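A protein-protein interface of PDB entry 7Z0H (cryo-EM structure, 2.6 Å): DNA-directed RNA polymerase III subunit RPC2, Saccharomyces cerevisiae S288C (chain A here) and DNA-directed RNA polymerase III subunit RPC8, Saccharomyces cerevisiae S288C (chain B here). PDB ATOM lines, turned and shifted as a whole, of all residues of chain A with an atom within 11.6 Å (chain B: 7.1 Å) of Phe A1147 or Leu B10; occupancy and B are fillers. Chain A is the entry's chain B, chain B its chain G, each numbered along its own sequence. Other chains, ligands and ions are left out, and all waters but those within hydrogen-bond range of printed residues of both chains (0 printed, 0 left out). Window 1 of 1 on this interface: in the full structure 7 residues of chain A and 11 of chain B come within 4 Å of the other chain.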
ATOM      1  N   ILE A1117       6.367  -8.486  13.014  1.00  0.00           N
ATOM      2  CA  ILE A1117       6.403  -8.672  14.459  1.00  0.00           C
ATOM      3  C   ILE A1117       5.155  -9.441  14.867  1.00  0.00           C
ATOM      4  O   ILE A1117       4.276  -9.703  14.039  1.00  0.00           O
ATOM      5  CB  ILE A1117       6.503  -7.335  15.211  1.00  0.00           C
ATOM      6  CG1 ILE A1117       5.218  -6.531  15.041  1.00  0.00           C
ATOM      7  CG2 ILE A1117       7.702  -6.534  14.729  1.00  0.00           C
ATOM      8  CD1 ILE A1117       4.775  -5.869  16.308  1.00  0.00           C
ATOM      9  N   LYS A1118       5.065  -9.803  16.142  1.00  0.00           N
ATOM     10  CA  LYS A1118       4.052 -10.735  16.619  1.00  0.00           C
ATOM     11  C   LYS A1118       3.306 -10.095  17.779  1.00  0.00           C
ATOM     12  O   LYS A1118       3.933  -9.616  18.730  1.00  0.00           O
ATOM     13  CB  LYS A1118       4.708 -12.054  17.042  1.00  0.00           C
ATOM     14  CG  LYS A1118       3.815 -13.271  16.969  1.00  0.00           C
ATOM     15  CD  LYS A1118       4.639 -14.546  16.869  1.00  0.00           C
ATOM     16  CE  LYS A1118       3.855 -15.668  16.206  1.00  0.00           C
ATOM     17  NZ  LYS A1118       2.697 -15.159  15.423  1.00  0.00           N
ATOM     18  N   MET A1119       1.975 -10.082  17.704  1.00  0.00           N
ATOM     19  CA  MET A1119       1.162  -9.476  18.750  1.00  0.00           C
ATOM     20  C   MET A1119      -0.209 -10.139  18.776  1.00  0.00           C
ATOM     21  O   MET A1119      -0.601 -10.846  17.845  1.00  0.00           O
ATOM     22  CB  MET A1119       1.018  -7.965  18.553  1.00  0.00           C
ATOM     23  CG  MET A1119       0.722  -7.543  17.127  1.00  0.00           C
ATOM     24  SD  MET A1119       1.316  -5.881  16.776  1.00  0.00           S
ATOM     25  CE  MET A1119       0.838  -5.024  18.274  1.00  0.00           C
ATOM     26  N   LEU A1143       3.106   0.715  14.773  1.00  0.00           N
ATOM     27  CA  LEU A1143       3.534  -0.002  15.965  1.00  0.00           C
ATOM     28  C   LEU A1143       4.697   0.722  16.621  1.00  0.00           C
ATOM     29  O   LEU A1143       5.591   1.222  15.931  1.00  0.00           O
ATOM     30  CB  LEU A1143       3.938  -1.435  15.610  1.00  0.00           C
ATOM     31  CG  LEU A1143       2.959  -2.152  14.677  1.00  0.00           C
ATOM     32  CD1 LEU A1143       3.613  -3.358  14.033  1.00  0.00           C
ATOM     33  CD2 LEU A1143       1.697  -2.553  15.422  1.00  0.00           C
ATOM     34  N   GLU A1144       4.680   0.776  17.950  1.00  0.00           N
ATOM     35  CA  GLU A1144       5.787   1.299  18.733  1.00  0.00           C
ATOM     36  C   GLU A1144       6.108   0.316  19.849  1.00  0.00           C
ATOM     37  O   GLU A1144       5.287  -0.530  20.212  1.00  0.00           O
ATOM     38  CB  GLU A1144       5.476   2.674  19.337  1.00  0.00           C
ATOM     39  CG  GLU A1144       4.259   2.696  20.240  1.00  0.00           C
ATOM     40  CD  GLU A1144       4.214   3.931  21.117  1.00  0.00           C
ATOM     41  OE1 GLU A1144       3.195   4.139  21.805  1.00  0.00           O
ATOM     42  OE2 GLU A1144       5.203   4.696  21.119  1.00  0.00           O
ATOM     43  N   ASP A1145       7.316   0.435  20.387  1.00  0.00           N
ATOM     44  CA  ASP A1145       7.725  -0.426  21.486  1.00  0.00           C
ATOM     45  C   ASP A1145       7.035  -0.009  22.778  1.00  0.00           C
ATOM     46  O   ASP A1145       6.919   1.180  23.084  1.00  0.00           O
ATOM     47  CB  ASP A1145       9.241  -0.378  21.665  1.00  0.00           C
ATOM     48  CG  ASP A1145       9.987  -0.537  20.358  1.00  0.00           C
ATOM     49  OD1 ASP A1145       9.598  -1.410  19.554  1.00  0.00           O
ATOM     50  OD2 ASP A1145      10.961   0.212  20.133  1.00  0.00           O
ATOM     51  N   ILE A1146       6.565  -1.003  23.532  1.00  0.00           N
ATOM     52  CA  ILE A1146       6.041  -0.738  24.869  1.00  0.00           C
ATOM     53  C   ILE A1146       7.145  -0.196  25.765  1.00  0.00           C
ATOM     54  O   ILE A1146       6.922   0.708  26.580  1.00  0.00           O
ATOM     55  CB  ILE A1146       5.416  -2.016  25.461  1.00  0.00           C
ATOM     56  CG1 ILE A1146       4.441  -2.651  24.469  1.00  0.00           C
ATOM     57  CG2 ILE A1146       4.725  -1.713  26.780  1.00  0.00           C
ATOM     58  CD1 ILE A1146       3.985  -4.036  24.867  1.00  0.00           C
ATOM     59  N   PHE A1147       8.348  -0.733  25.619  1.00  0.00           N
ATOM     60  CA  PHE A1147       9.477  -0.423  26.481  1.00  0.00           C
ATOM     61  C   PHE A1147      10.340   0.656  25.822  1.00  0.00           C
ATOM     62  O   PHE A1147       9.897   1.332  24.890  1.00  0.00           O
ATOM     63  CB  PHE A1147      10.236  -1.712  26.794  1.00  0.00           C
ATOM     64  CG  PHE A1147       9.385  -2.755  27.448  1.00  0.00           C
ATOM     65  CD1 PHE A1147       8.724  -2.480  28.631  1.00  0.00           C
ATOM     66  CD2 PHE A1147       9.224  -4.001  26.873  1.00  0.00           C
ATOM     67  CE1 PHE A1147       7.934  -3.430  29.237  1.00  0.00           C
ATOM     68  CE2 PHE A1147       8.431  -4.955  27.475  1.00  0.00           C
ATOM     69  CZ  PHE A1147       7.786  -4.668  28.658  1.00  0.00           C
ATOM     70  N   GLN A1148      11.559   0.853  26.343  1.00  0.00           N
ATOM     71  CA  GLN A1148      12.518   1.878  25.928  1.00  0.00           C
ATOM     72  C   GLN A1148      12.096   3.236  26.479  1.00  0.00           C
ATOM     73  O   GLN A1148      12.812   4.229  26.320  1.00  0.00           O
ATOM     74  CB  GLN A1148      12.679   1.919  24.401  1.00  0.00           C
ATOM     75  CG  GLN A1148      13.888   2.700  23.895  1.00  0.00           C
ATOM     76  CD  GLN A1148      15.129   2.479  24.739  1.00  0.00           C
ATOM     77  OE1 GLN A1148      15.407   3.238  25.668  1.00  0.00           O
ATOM     78  NE2 GLN A1148      15.884   1.436  24.417  1.00  0.00           N
ATOM     79  N   GLN A1149      10.943   3.276  27.141  1.00  0.00           N
ATOM     80  CA  GLN A1149      10.503   4.443  27.898  1.00  0.00           C
ATOM     81  C   GLN A1149      10.411   5.699  27.034  1.00  0.00           C
ATOM     82  O   GLN A1149       9.358   6.004  26.476  1.00  0.00           O
ATOM     83  CB  GLN A1149      11.449   4.681  29.076  1.00  0.00           C
ATOM     84  CG  GLN A1149      10.847   5.469  30.219  1.00  0.00           C
ATOM     85  CD  GLN A1149      11.699   5.399  31.469  1.00  0.00           C
ATOM     86  OE1 GLN A1149      12.863   5.002  31.422  1.00  0.00           O
ATOM     87  NE2 GLN A1149      11.116   5.771  32.599  1.00  0.00           N
ATOM     88  N   ALA B   8      23.443  -2.408  22.886  1.00  0.00           N
ATOM     89  CA  ALA B   8      22.300  -2.057  23.715  1.00  0.00           C
ATOM     90  C   ALA B   8      21.160  -3.013  23.397  1.00  0.00           C
ATOM     91  O   ALA B   8      20.821  -3.206  22.225  1.00  0.00           O
ATOM     92  CB  ALA B   8      21.868  -0.609  23.474  1.00  0.00           C
ATOM     93  N   ASP B   9      20.575  -3.611  24.432  1.00  0.00           N
ATOM     94  CA  ASP B   9      19.533  -4.605  24.226  1.00  0.00           C
ATOM     95  C   ASP B   9      18.565  -4.596  25.397  1.00  0.00           C
ATOM     96  O   ASP B   9      18.859  -4.072  26.474  1.00  0.00           O
ATOM     97  CB  ASP B   9      20.123  -6.007  24.037  1.00  0.00           C
ATOM     98  CG  ASP B   9      19.184  -6.936  23.295  1.00  0.00           C
ATOM     99  OD1 ASP B   9      18.108  -6.473  22.860  1.00  0.00           O
ATOM    100  OD2 ASP B   9      19.519  -8.130  23.150  1.00  0.00           O
ATOM    101  N   LEU B  10      17.396  -5.189  25.163  1.00  0.00           N
ATOM    102  CA  LEU B  10      16.341  -5.331  26.160  1.00  0.00           C
ATOM    103  C   LEU B  10      16.273  -6.798  26.565  1.00  0.00           C
ATOM    104  O   LEU B  10      15.943  -7.659  25.742  1.00  0.00           O
ATOM    105  CB  LEU B  10      15.005  -4.851  25.599  1.00  0.00           C
ATOM    106  CG  LEU B  10      13.749  -5.012  26.457  1.00  0.00           C
ATOM    107  CD1 LEU B  10      13.701  -3.970  27.563  1.00  0.00           C
ATOM    108  CD2 LEU B  10      12.504  -4.941  25.590  1.00  0.00           C
ATOM    109  N   VAL B  11      16.583  -7.083  27.826  1.00  0.00           N
ATOM    110  CA  VAL B  11      16.541  -8.442  28.351  1.00  0.00           C
ATOM    111  C   VAL B  11      15.297  -8.598  29.207  1.00  0.00           C
ATOM    112  O   VAL B  11      14.816  -7.643  29.827  1.00  0.00           O
ATOM    113  CB  VAL B  11      17.811  -8.792  29.156  1.00  0.00           C
ATOM    114  CG1 VAL B  11      18.949  -9.140  28.221  1.00  0.00           C
ATOM    115  CG2 VAL B  11      18.195  -7.644  30.072  1.00  0.00           C
ATOM    116  N   ARG B  12      14.772  -9.819  29.246  1.00  0.00           N
ATOM    117  CA  ARG B  12      13.558 -10.140  29.986  1.00  0.00           C
ATOM    118  C   ARG B  12      13.910 -11.148  31.071  1.00  0.00           C
ATOM    119  O   ARG B  12      14.194 -12.313  30.775  1.00  0.00           O
ATOM    120  CB  ARG B  12      12.484 -10.684  29.046  1.00  0.00           C
ATOM    121  CG  ARG B  12      11.300 -11.333  29.734  1.00  0.00           C
ATOM    122  CD  ARG B  12      10.392 -11.997  28.715  1.00  0.00           C
ATOM    123  NE  ARG B  12       9.350 -12.801  29.336  1.00  0.00           N
ATOM    124  CZ  ARG B  12       9.521 -14.044  29.767  1.00  0.00           C
ATOM    125  NH1 ARG B  12      10.691 -14.654  29.669  1.00  0.00           N
ATOM    126  NH2 ARG B  12       8.493 -14.690  30.309  1.00  0.00           N
ATOM    127  N   LEU B  30      21.610 -12.475  28.526  1.00  0.00           N
ATOM    128  CA  LEU B  30      22.420 -12.025  27.401  1.00  0.00           C
ATOM    129  C   LEU B  30      23.235 -13.168  26.813  1.00  0.00           C
ATOM    130  O   LEU B  30      23.482 -13.193  25.605  1.00  0.00           O
ATOM    131  CB  LEU B  30      23.331 -10.882  27.842  1.00  0.00           C
ATOM    132  CG  LEU B  30      22.657  -9.512  27.896  1.00  0.00           C
ATOM    133  CD1 LEU B  30      23.620  -8.461  28.412  1.00  0.00           C
ATOM    134  CD2 LEU B  30      22.129  -9.132  26.526  1.00  0.00           C
ATOM    135  N   LYS B  33      21.027 -15.285  24.722  1.00  0.00           N
ATOM    136  CA  LYS B  33      20.769 -14.621  23.450  1.00  0.00           C
ATOM    137  C   LYS B  33      22.006 -14.498  22.564  1.00  0.00           C
ATOM    138  O   LYS B  33      21.861 -14.312  21.351  1.00  0.00           O
ATOM    139  CB  LYS B  33      20.177 -13.227  23.678  1.00  0.00           C
ATOM    140  CG  LYS B  33      19.180 -12.817  22.606  1.00  0.00           C
ATOM    141  CD  LYS B  33      19.171 -11.316  22.386  1.00  0.00           C
ATOM    142  CE  LYS B  33      18.119 -10.920  21.364  1.00  0.00           C
ATOM    143  NZ  LYS B  33      18.004  -9.442  21.231  1.00  0.00           N
ATOM    144  N   GLY B  57      14.073  -2.135  35.552  1.00  0.00           N
ATOM    145  CA  GLY B  57      13.249  -3.051  34.781  1.00  0.00           C
ATOM    146  C   GLY B  57      11.789  -2.643  34.826  1.00  0.00           C
ATOM    147  O   GLY B  57      11.242  -2.350  35.895  1.00  0.00           O
ATOM    148  N   GLN B  58      11.148  -2.631  33.663  1.00  0.00           N
ATOM    149  CA  GLN B  58       9.756  -2.232  33.538  1.00  0.00           C
ATOM    150  C   GLN B  58       8.914  -3.424  33.106  1.00  0.00           C
ATOM    151  O   GLN B  58       9.394  -4.329  32.419  1.00  0.00           O
ATOM    152  CB  GLN B  58       9.595  -1.082  32.540  1.00  0.00           C
ATOM    153  CG  GLN B  58      10.436  -1.234  31.293  1.00  0.00           C
ATOM    154  CD  GLN B  58      10.651   0.079  30.574  1.00  0.00           C
ATOM    155  OE1 GLN B  58      10.051   1.095  30.920  1.00  0.00           O
ATOM    156  NE2 GLN B  58      11.516   0.066  29.568  1.00  0.00           N
ATOM    157  N   LEU B  59       7.651  -3.413  33.519  1.00  0.00           N
ATOM    158  CA  LEU B  59       6.740  -4.528  33.314  1.00  0.00           C
ATOM    159  C   LEU B  59       5.615  -4.112  32.378  1.00  0.00           C
ATOM    160  O   LEU B  59       4.953  -3.095  32.613  1.00  0.00           O
ATOM    161  CB  LEU B  59       6.155  -5.003  34.644  1.00  0.00           C
ATOM    162  CG  LEU B  59       7.095  -5.706  35.621  1.00  0.00           C
ATOM    163  CD1 LEU B  59       7.758  -4.710  36.555  1.00  0.00           C
ATOM    164  CD2 LEU B  59       6.333  -6.746  36.409  1.00  0.00           C
ATOM    165  N   LYS B  60       5.402  -4.893  31.323  1.00  0.00           N
ATOM    166  CA  LYS B  60       4.196  -4.731  30.535  1.00  0.00           C
ATOM    167  C   LYS B  60       3.005  -5.267  31.327  1.00  0.00           C
ATOM    168  O   LYS B  60       3.160  -6.157  32.166  1.00  0.00           O
ATOM    169  CB  LYS B  60       4.317  -5.451  29.193  1.00  0.00           C
ATOM    170  CG  LYS B  60       4.626  -6.928  29.284  1.00  0.00           C
ATOM    171  CD  LYS B  60       5.269  -7.423  28.001  1.00  0.00           C
ATOM    172  CE  LYS B  60       4.238  -8.015  27.059  1.00  0.00           C
ATOM    173  NZ  LYS B  60       4.855  -8.510  25.798  1.00  0.00           N
ATOM    174  N   PRO B  61       1.804  -4.739  31.084  1.00  0.00           N
ATOM    175  CA  PRO B  61       0.663  -5.068  31.953  1.00  0.00           C
ATOM    176  C   PRO B  61       0.215  -6.523  31.914  1.00  0.00           C
ATOM    177  O   PRO B  61      -0.789  -6.859  32.546  1.00  0.00           O
ATOM    178  CB  PRO B  61      -0.445  -4.144  31.430  1.00  0.00           C
ATOM    179  CG  PRO B  61       0.273  -3.029  30.758  1.00  0.00           C
ATOM    180  CD  PRO B  61       1.477  -3.659  30.138  1.00  0.00           C
ATOM    181  N   ASP B  63       2.746  -9.532  31.455  1.00  0.00           N
ATOM    182  CA  ASP B  63       3.769 -10.565  31.574  1.00  0.00           C
ATOM    183  C   ASP B  63       4.163 -10.836  33.023  1.00  0.00           C
ATOM    184  O   ASP B  63       4.132 -11.985  33.469  1.00  0.00           O
ATOM    185  CB  ASP B  63       5.009 -10.177  30.762  1.00  0.00           C
ATOM    186  CG  ASP B  63       5.887 -11.371  30.430  1.00  0.00           C
ATOM    187  OD1 ASP B  63       5.587 -12.485  30.909  1.00  0.00           O
ATOM    188  OD2 ASP B  63       6.877 -11.195  29.691  1.00  0.00           O
ATOM    189  N   SER B  65       7.230 -10.398  34.020  1.00  0.00           N
ATOM    190  CA  SER B  65       8.681 -10.423  33.955  1.00  0.00           C
ATOM    191  C   SER B  65       9.234  -9.002  33.943  1.00  0.00           C
ATOM    192  O   SER B  65       8.543  -8.039  33.603  1.00  0.00           O
ATOM    193  CB  SER B  65       9.148 -11.178  32.712  1.00  0.00           C
ATOM    194  OG  SER B  65       8.293 -12.269  32.427  1.00  0.00           O
ATOM    195  N   SER B  66      10.501  -8.880  34.326  1.00  0.00           N
ATOM    196  CA  SER B  66      11.189  -7.597  34.328  1.00  0.00           C
ATOM    197  C   SER B  66      11.935  -7.427  33.011  1.00  0.00           C
ATOM    198  O   SER B  66      12.813  -8.230  32.681  1.00  0.00           O
ATOM    199  CB  SER B  66      12.151  -7.502  35.510  1.00  0.00           C
ATOM    200  OG  SER B  66      12.554  -6.164  35.734  1.00  0.00           O
ATOM    201  N   TYR B  67      11.583  -6.386  32.262  1.00  0.00           N
ATOM    202  CA  TYR B  67      12.247  -6.063  31.006  1.00  0.00           C
ATOM    203  C   TYR B  67      13.238  -4.937  31.262  1.00  0.00           C
ATOM    204  O   TYR B  67      12.841  -3.827  31.631  1.00  0.00           O
ATOM    205  CB  TYR B  67      11.236  -5.663  29.934  1.00  0.00           C
ATOM    206  CG  TYR B  67      10.377  -6.804  29.441  1.00  0.00           C
ATOM    207  CD1 TYR B  67       9.297  -7.258  30.187  1.00  0.00           C
ATOM    208  CD2 TYR B  67      10.644  -7.425  28.231  1.00  0.00           C
ATOM    209  CE1 TYR B  67       8.507  -8.295  29.739  1.00  0.00           C
ATOM    210  CE2 TYR B  67       9.860  -8.465  27.775  1.00  0.00           C
ATOM    211  CZ  TYR B  67       8.793  -8.895  28.534  1.00  0.00           C
ATOM    212  OH  TYR B  67       8.009  -9.932  28.086  1.00  0.00           O
ATOM    213  N   ILE B  68      14.521  -5.220  31.057  1.00  0.00           N
ATOM    214  CA  ILE B  68      15.600  -4.316  31.433  1.00  0.00           C
ATOM    215  C   ILE B  68      16.307  -3.847  30.172  1.00  0.00           C
ATOM    216  O   ILE B  68      16.793  -4.668  29.385  1.00  0.00           O
ATOM    217  CB  ILE B  68      16.592  -4.988  32.393  1.00  0.00           C
ATOM    218  CG1 ILE B  68      15.865  -5.502  33.637  1.00  0.00           C
ATOM    219  CG2 ILE B  68      17.703  -4.026  32.762  1.00  0.00           C
ATOM    220  CD1 ILE B  68      16.784  -5.893  34.763  1.00  0.00           C
ATOM    221  N   ASN B  69      16.366  -2.531  29.981  1.00  0.00           N
ATOM    222  CA  ASN B  69      17.218  -1.943  28.954  1.00  0.00           C
ATOM    223  C   ASN B  69      18.654  -1.991  29.457  1.00  0.00           C
ATOM    224  O   ASN B  69      18.979  -1.390  30.485  1.00  0.00           O
ATOM    225  CB  ASN B  69      16.790  -0.511  28.648  1.00  0.00           C
ATOM    226  CG  ASN B  69      15.578  -0.445  27.744  1.00  0.00           C
ATOM    227  OD1 ASN B  69      14.625   0.284  28.016  1.00  0.00           O
ATOM    228  ND2 ASN B  69      15.610  -1.207  26.658  1.00  0.00           N
ATOM    229  N   VAL B  70      19.515  -2.712  28.745  1.00  0.00           N
ATOM    230  CA  VAL B  70      20.885  -2.937  29.182  1.00  0.00           C
ATOM    231  C   VAL B  70      21.837  -2.658  28.028  1.00  0.00           C
ATOM    232  O   VAL B  70      21.564  -3.019  26.877  1.00  0.00           O
ATOM    233  CB  VAL B  70      21.080  -4.369  29.732  1.00  0.00           C
ATOM    234  CG1 VAL B  70      20.875  -5.410  28.643  1.00  0.00           C
ATOM    235  CG2 VAL B  70      22.457  -4.518  30.354  1.00  0.00           C
ATOM    236  N   PHE B  72      25.934  -3.369  27.098  1.00  0.00           N
ATOM    237  CA  PHE B  72      26.958  -4.296  27.546  1.00  0.00           C
ATOM    238  C   PHE B  72      28.068  -4.361  26.513  1.00  0.00           C
ATOM    239  O   PHE B  72      27.867  -4.065  25.333  1.00  0.00           O
ATOM    240  CB  PHE B  72      26.380  -5.694  27.797  1.00  0.00           C
ATOM    241  CG  PHE B  72      25.812  -6.347  26.567  1.00  0.00           C
ATOM    242  CD1 PHE B  72      24.577  -5.969  26.071  1.00  0.00           C
ATOM    243  CD2 PHE B  72      26.514  -7.342  25.910  1.00  0.00           C
ATOM    244  CE1 PHE B  72      24.053  -6.567  24.943  1.00  0.00           C
ATOM    245  CE2 PHE B  72      25.995  -7.945  24.780  1.00  0.00           C
ATOM    246  CZ  PHE B  72      24.762  -7.556  24.297  1.00  0.00           C
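Leu B10 touches Phe A1147. CD1 of Phe A1147 touches CG of Gln B58, at 3.4 Å. Leu B59 touches Phe A1147. Phe A1147 touches Lys B60. Phe A1147 touches Tyr B67.
Printed residues of chain A that touch a printed residue of chain B: Phe A1147 and Gln A1148. Hydrophobic or aromatic side chains of chain A that line the printed part of chain B: Phe A1147. Of the 20 printed residues of chain B, 6 touch a printed residue of chain A. Hydrophobic or aromatic side chains of chain B within 4 Å of the printed part of chain A: Leu B10 and Tyr B67.
OD1 of Asn B69 is in hydrogen-bond range of NE2 of Gln B58. OH of Tyr B67 lies close to NE of Arg B12. The backbone NH of Gln B58 lies within hydrogen-bond range of the backbone carbonyl oxygen of Tyr B67, at 2.9 Å.
NE2 of Gln A1148 lies close to ND2 of Asn B69, 3.5 Å away. NE2 of Gln B58 sits close to N of Gln A1148, at 3.3 Å.
Of chain B, only Leu B10 (3.6 Å), Gln B58 (3.4 Å), Leu B59 (3.96 Å), Lys B60 (3.6 Å) and Tyr B67 (3.3 Å) come within 4 Å of Phe A1147. Printed residues of chain A within 4 Å of Leu B10: Phe A1147. Ala B8 touches none of the printed residues of chain A. No residue of chain A comes within 4 Å of Val B11. Of the printed residues of chain A, Gln B58 touches Phe A1147 and Gln A1148. Lys B60 touches one residue of chain A. Printed residues of chain A within 4 Å of Tyr B67: Phe A1147. Of chain A, only Gln A1148 (3.4 Å) comes within 4 Å of Asn B69. Of the printed residues of chain B, Gln A1148 touches Gln B58 and Asn B69. Of the printed residues of chain A, Leu B59 touches Phe A1147 (3.96 Å). The nearest printed residue of chain A that does not touch Leu B59 is Ile A1146 (6.0 Å).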
